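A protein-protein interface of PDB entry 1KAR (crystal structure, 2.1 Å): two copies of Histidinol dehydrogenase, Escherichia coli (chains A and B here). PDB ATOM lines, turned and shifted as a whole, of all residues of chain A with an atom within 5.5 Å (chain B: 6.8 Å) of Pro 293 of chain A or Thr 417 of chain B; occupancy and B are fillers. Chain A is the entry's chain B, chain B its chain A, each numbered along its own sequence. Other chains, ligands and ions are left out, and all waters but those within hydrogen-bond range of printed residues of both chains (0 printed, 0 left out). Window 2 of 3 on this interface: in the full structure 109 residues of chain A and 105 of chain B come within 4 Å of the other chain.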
ATOM      1  N   GLU A 261     -15.464   4.141  12.183  1.00  0.00           N
ATOM      2  CA  GLU A 261     -16.710   4.878  12.002  1.00  0.00           C
ATOM      3  C   GLU A 261     -17.019   5.198  10.541  1.00  0.00           C
ATOM      4  O   GLU A 261     -18.050   5.788  10.240  1.00  0.00           O
ATOM      5  CB  GLU A 261     -16.733   6.166  12.854  1.00  0.00           C
ATOM      6  CG  GLU A 261     -15.723   7.248  12.476  1.00  0.00           C
ATOM      7  CD  GLU A 261     -16.001   8.573  13.180  1.00  0.00           C
ATOM      8  OE1 GLU A 261     -16.801   8.596  14.131  1.00  0.00           O
ATOM      9  OE2 GLU A 261     -15.417   9.590  12.784  1.00  0.00           O
ATOM     10  N   GLU A 291     -18.382   7.025  24.366  1.00  0.00           N
ATOM     11  CA  GLU A 291     -18.659   8.452  24.225  1.00  0.00           C
ATOM     12  C   GLU A 291     -19.083   8.865  22.825  1.00  0.00           C
ATOM     13  O   GLU A 291     -19.500  10.003  22.606  1.00  0.00           O
ATOM     14  CB  GLU A 291     -17.438   9.281  24.636  1.00  0.00           C
ATOM     15  CG  GLU A 291     -17.152   9.248  26.122  1.00  0.00           C
ATOM     16  CD  GLU A 291     -16.232  10.366  26.570  1.00  0.00           C
ATOM     17  OE1 GLU A 291     -16.650  11.541  26.535  1.00  0.00           O
ATOM     18  OE2 GLU A 291     -15.089  10.072  26.963  1.00  0.00           O
ATOM     19  N   LEU A 292     -18.976   7.950  21.868  1.00  0.00           N
ATOM     20  CA  LEU A 292     -19.362   8.275  20.504  1.00  0.00           C
ATOM     21  C   LEU A 292     -20.884   8.340  20.375  1.00  0.00           C
ATOM     22  O   LEU A 292     -21.588   7.345  20.590  1.00  0.00           O
ATOM     23  CB  LEU A 292     -18.775   7.252  19.527  1.00  0.00           C
ATOM     24  CG  LEU A 292     -17.246   7.257  19.417  1.00  0.00           C
ATOM     25  CD1 LEU A 292     -16.825   6.311  18.300  1.00  0.00           C
ATOM     26  CD2 LEU A 292     -16.745   8.660  19.128  1.00  0.00           C
ATOM     27  N   PRO A 293     -21.407   9.523  20.010  1.00  0.00           N
ATOM     28  CA  PRO A 293     -22.839   9.779  19.844  1.00  0.00           C
ATOM     29  C   PRO A 293     -23.572   8.597  19.245  1.00  0.00           C
ATOM     30  O   PRO A 293     -24.403   7.966  19.899  1.00  0.00           O
ATOM     31  CB  PRO A 293     -22.866  11.000  18.932  1.00  0.00           C
ATOM     32  CG  PRO A 293     -21.663  11.747  19.365  1.00  0.00           C
ATOM     33  CD  PRO A 293     -20.620  10.653  19.484  1.00  0.00           C
ATOM     34  N   ARG A 294     -23.250   8.296  17.995  1.00  0.00           N
ATOM     35  CA  ARG A 294     -23.877   7.190  17.300  1.00  0.00           C
ATOM     36  C   ARG A 294     -22.776   6.349  16.696  1.00  0.00           C
ATOM     37  O   ARG A 294     -22.375   6.551  15.554  1.00  0.00           O
ATOM     38  CB  ARG A 294     -24.815   7.731  16.220  1.00  0.00           C
ATOM     39  CG  ARG A 294     -24.279   8.948  15.482  1.00  0.00           C
ATOM     40  CD  ARG A 294     -25.326   9.484  14.527  1.00  0.00           C
ATOM     41  NE  ARG A 294     -24.852  10.640  13.772  1.00  0.00           N
ATOM     42  CZ  ARG A 294     -25.562  11.259  12.830  1.00  0.00           C
ATOM     43  NH1 ARG A 294     -26.783  10.832  12.527  1.00  0.00           N
ATOM     44  NH2 ARG A 294     -25.052  12.307  12.194  1.00  0.00           N
ATOM     45  N   ALA A 295     -22.289   5.398  17.482  1.00  0.00           N
ATOM     46  CA  ALA A 295     -21.203   4.538  17.048  1.00  0.00           C
ATOM     47  C   ALA A 295     -21.613   3.097  16.769  1.00  0.00           C
ATOM     48  O   ALA A 295     -20.822   2.180  16.984  1.00  0.00           O
ATOM     49  CB  ALA A 295     -20.100   4.567  18.087  1.00  0.00           C
ATOM     50  N   ALA B 411     -13.846  17.783  10.265  1.00  0.00           N
ATOM     51  CA  ALA B 411     -14.371  16.522  10.765  1.00  0.00           C
ATOM     52  C   ALA B 411     -15.757  16.767  11.369  1.00  0.00           C
ATOM     53  O   ALA B 411     -16.673  15.949  11.223  1.00  0.00           O
ATOM     54  CB  ALA B 411     -13.418  15.933  11.808  1.00  0.00           C
ATOM     55  N   ALA B 412     -15.911  17.911  12.028  1.00  0.00           N
ATOM     56  CA  ALA B 412     -17.177  18.263  12.644  1.00  0.00           C
ATOM     57  C   ALA B 412     -18.264  18.452  11.587  1.00  0.00           C
ATOM     58  O   ALA B 412     -19.378  17.981  11.757  1.00  0.00           O
ATOM     59  CB  ALA B 412     -17.023  19.531  13.485  1.00  0.00           C
ATOM     60  N   GLU B 414     -18.497  17.023   8.781  1.00  0.00           N
ATOM     61  CA  GLU B 414     -18.837  15.744   8.159  1.00  0.00           C
ATOM     62  C   GLU B 414     -19.438  14.788   9.188  1.00  0.00           C
ATOM     63  O   GLU B 414     -19.690  13.622   8.895  1.00  0.00           O
ATOM     64  CB  GLU B 414     -17.603  15.094   7.516  1.00  0.00           C
ATOM     65  CG  GLU B 414     -16.976  15.904   6.389  1.00  0.00           C
ATOM     66  CD  GLU B 414     -16.022  15.079   5.527  1.00  0.00           C
ATOM     67  OE1 GLU B 414     -15.460  14.082   6.039  1.00  0.00           O
ATOM     68  OE2 GLU B 414     -15.823  15.435   4.338  1.00  0.00           O
ATOM     69  N   ARG B 415     -19.672  15.288  10.395  1.00  0.00           N
ATOM     70  CA  ARG B 415     -20.247  14.476  11.463  1.00  0.00           C
ATOM     71  C   ARG B 415     -19.395  13.255  11.804  1.00  0.00           C
ATOM     72  O   ARG B 415     -19.928  12.176  12.086  1.00  0.00           O
ATOM     73  CB  ARG B 415     -21.652  14.002  11.084  1.00  0.00           C
ATOM     74  CG  ARG B 415     -22.617  15.105  10.717  1.00  0.00           C
ATOM     75  CD  ARG B 415     -23.662  15.314  11.798  1.00  0.00           C
ATOM     76  NE  ARG B 415     -24.933  15.732  11.213  1.00  0.00           N
ATOM     77  CZ  ARG B 415     -25.692  14.950  10.446  1.00  0.00           C
ATOM     78  NH1 ARG B 415     -25.312  13.705  10.176  1.00  0.00           N
ATOM     79  NH2 ARG B 415     -26.823  15.417   9.935  1.00  0.00           N
ATOM     80  N   LEU B 416     -18.076  13.418  11.774  1.00  0.00           N
ATOM     81  CA  LEU B 416     -17.185  12.311  12.103  1.00  0.00           C
ATOM     82  C   LEU B 416     -16.546  12.585  13.460  1.00  0.00           C
ATOM     83  O   LEU B 416     -15.418  13.072  13.558  1.00  0.00           O
ATOM     84  CB  LEU B 416     -16.123  12.142  11.010  1.00  0.00           C
ATOM     85  CG  LEU B 416     -16.709  11.733   9.646  1.00  0.00           C
ATOM     86  CD1 LEU B 416     -15.642  11.788   8.582  1.00  0.00           C
ATOM     87  CD2 LEU B 416     -17.310  10.328   9.744  1.00  0.00           C
ATOM     88  N   THR B 417     -17.303  12.262  14.503  1.00  0.00           N
ATOM     89  CA  THR B 417     -16.899  12.465  15.888  1.00  0.00           C
ATOM     90  C   THR B 417     -15.533  11.868  16.237  1.00  0.00           C
ATOM     91  O   THR B 417     -14.660  12.569  16.762  1.00  0.00           O
ATOM     92  CB  THR B 417     -17.956  11.876  16.816  1.00  0.00           C
ATOM     93  OG1 THR B 417     -19.253  12.173  16.284  1.00  0.00           O
ATOM     94  CG2 THR B 417     -17.837  12.483  18.206  1.00  0.00           C
ATOM     95  N   ALA B 418     -15.349  10.580  15.957  1.00  0.00           N
ATOM     96  CA  ALA B 418     -14.073   9.927  16.243  1.00  0.00           C
ATOM     97  C   ALA B 418     -12.935  10.639  15.511  1.00  0.00           C
ATOM     98  O   ALA B 418     -11.832  10.744  16.040  1.00  0.00           O
ATOM     99  CB  ALA B 418     -14.115   8.430  15.841  1.00  0.00           C
ATOM    100  N   HIS B 419     -13.188  11.111  14.293  1.00  0.00           N
ATOM    101  CA  HIS B 419     -12.150  11.830  13.546  1.00  0.00           C
ATOM    102  C   HIS B 419     -11.816  13.113  14.288  1.00  0.00           C
ATOM    103  O   HIS B 419     -10.662  13.532  14.335  1.00  0.00           O
ATOM    104  CB  HIS B 419     -12.620  12.207  12.131  1.00  0.00           C
ATOM    105  CG  HIS B 419     -12.496  11.106  11.119  1.00  0.00           C
ATOM    106  ND1 HIS B 419     -13.229   9.942  11.188  1.00  0.00           N
ATOM    107  CD2 HIS B 419     -11.763  11.022   9.984  1.00  0.00           C
ATOM    108  CE1 HIS B 419     -12.959   9.190  10.135  1.00  0.00           C
ATOM    109  NE2 HIS B 419     -12.072   9.823   9.390  1.00  0.00           N
ATOM    110  N   LYS B 420     -12.834  13.759  14.848  1.00  0.00           N
ATOM    111  CA  LYS B 420     -12.594  14.995  15.577  1.00  0.00           C
ATOM    112  C   LYS B 420     -11.907  14.706  16.920  1.00  0.00           C
ATOM    113  O   LYS B 420     -10.973  15.411  17.311  1.00  0.00           O
ATOM    114  CB  LYS B 420     -13.906  15.765  15.796  1.00  0.00           C
ATOM    115  CG  LYS B 420     -13.766  16.911  16.794  1.00  0.00           C
ATOM    116  CD  LYS B 420     -14.930  17.882  16.723  1.00  0.00           C
ATOM    117  CE  LYS B 420     -15.052  18.672  18.022  1.00  0.00           C
ATOM    118  NZ  LYS B 420     -13.742  19.204  18.506  1.00  0.00           N
ATOM    119  N   ASN B 421     -12.352  13.655  17.606  1.00  0.00           N
ATOM    120  CA  ASN B 421     -11.768  13.287  18.891  1.00  0.00           C
ATOM    121  C   ASN B 421     -10.295  12.920  18.822  1.00  0.00           C
ATOM    122  O   ASN B 421      -9.581  13.125  19.797  1.00  0.00           O
ATOM    123  CB  ASN B 421     -12.530  12.123  19.528  1.00  0.00           C
ATOM    124  CG  ASN B 421     -13.923  12.517  19.983  1.00  0.00           C
ATOM    125  OD1 ASN B 421     -14.295  13.695  19.945  1.00  0.00           O
ATOM    126  ND2 ASN B 421     -14.699  11.536  20.423  1.00  0.00           N
ATOM    127  N   ALA B 422      -9.837  12.377  17.690  1.00  0.00           N
ATOM    128  CA  ALA B 422      -8.430  12.003  17.552  1.00  0.00           C
ATOM    129  C   ALA B 422      -7.583  13.261  17.625  1.00  0.00           C
ATOM    130  O   ALA B 422      -6.435  13.232  18.064  1.00  0.00           O
ATOM    131  CB  ALA B 422      -8.181  11.282  16.208  1.00  0.00           C
ATOM    132  N   VAL B 423      -8.159  14.368  17.187  1.00  0.00           N
ATOM    133  CA  VAL B 423      -7.467  15.643  17.212  1.00  0.00           C
ATOM    134  C   VAL B 423      -7.496  16.237  18.622  1.00  0.00           C
ATOM    135  O   VAL B 423      -6.460  16.654  19.152  1.00  0.00           O
ATOM    136  CB  VAL B 423      -8.125  16.632  16.218  1.00  0.00           C
ATOM    137  CG1 VAL B 423      -7.428  17.992  16.272  1.00  0.00           C
ATOM    138  CG2 VAL B 423      -8.077  16.036  14.800  1.00  0.00           C
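The guanidinium group (NH1) of Arg 415 of chain B lies close to the guanidinium group (NH2) of Arg 294 of chain A (2.5 Å).
The side-chain carboxylate (OE1) of Glu 261 of chain A lies within hydrogen-bond range of the backbone NH (N) of Ala 418 of chain B.
A ring nitrogen (ND1) of His 419 of chain B is in hydrogen-bond range of the side-chain carboxylate (OE2) of Glu 261 of chain A, 2.7 Å away.
The backbone carbonyl oxygen (O) of Ala 411 of chain B sits at hydrogen-bond distance from the backbone NH (N) of Leu 416 of chain B.
The backbone carbonyl oxygen (O) of Thr 417 of chain B lies close to the side-chain amide oxygen (OD1) of Asn 421 of chain B (3.4 Å).
Glu 261 of chain A touches Leu 416 of chain B.
Thr 417 of chain B touches Glu 261 of chain A.
CD2 of Leu 292 of chain A touches N of Ala 418 of chain B, at 3.96 Å.
Leu 292 of chain A touches Asn 421 of chain B (CD2 to ND2, 3.8 Å).
Pro 293 of chain A touches Thr 417 of chain B (CD to CG2, 3.6 Å).
Of chain B, only Thr 417 comes within 4 Å of Pro 293 of chain A.
Thr 417 of chain B touches just these residues of chain A: Glu 261 (3.7 Å) and Pro 293 (3.6 Å).
Of the printed residues of chain A, Asn 421 of chain B touches Leu 292 (3.8 Å).
Printed residues of chain A within 4 Å of His 419 of chain B: Glu 261 (2.7 Å).
Of the printed residues of chain A, Arg 415 of chain B touches Arg 294 (2.5 Å).
Printed residues of chain B within 4 Å of Leu 292 of chain A: Ala 418 (3.96 Å) and Asn 421 (3.8 Å).
Of the printed residues of chain A, Leu 416 of chain B touches Glu 261.
Glu 291 of chain A touches none of the printed residues of chain B.
Ala 412 of chain B touches none of the printed residues of chain A.
The nearest residue of chain A that does not touch Thr 417 of chain B is Leu 292 of chain A (4.1 Å).
The nearest printed residue of chain A that does not touch Asn 421 of chain B is Glu 291 of chain A (5.5 Å).
Printed residues of chain B that touch a printed residue of chain A: Arg 415, Leu 416, Thr 417, Ala 418, His 419 and Asn 421.
Hydrophobic or aromatic side chains of chain B within 4 Å of the printed part of chain A: Leu 416, Ala 418 and His 419.
Of the 6 printed residues of chain A, 4 touch a printed residue of chain B.
Printed residues of chain A that touch a printed residue of chain B: Glu 261, Leu 292, Pro 293 and Arg 294.
Hydrophobic or aromatic side chains of chain A within 4 Å of the printed part of chain B: Leu 292 and Pro 293.
Among the printed residues, 8 pairs touch across the chains.
Among the printed residues, no Asp or Glu carboxylate lies within 4 Å of a Lys or Arg side-chain nitrogen of the other chain.
No position is printed for both chains.
Of the 8 pairs that touch across the chains among the printed residues, none has its exchanged pair printed and touching as well.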
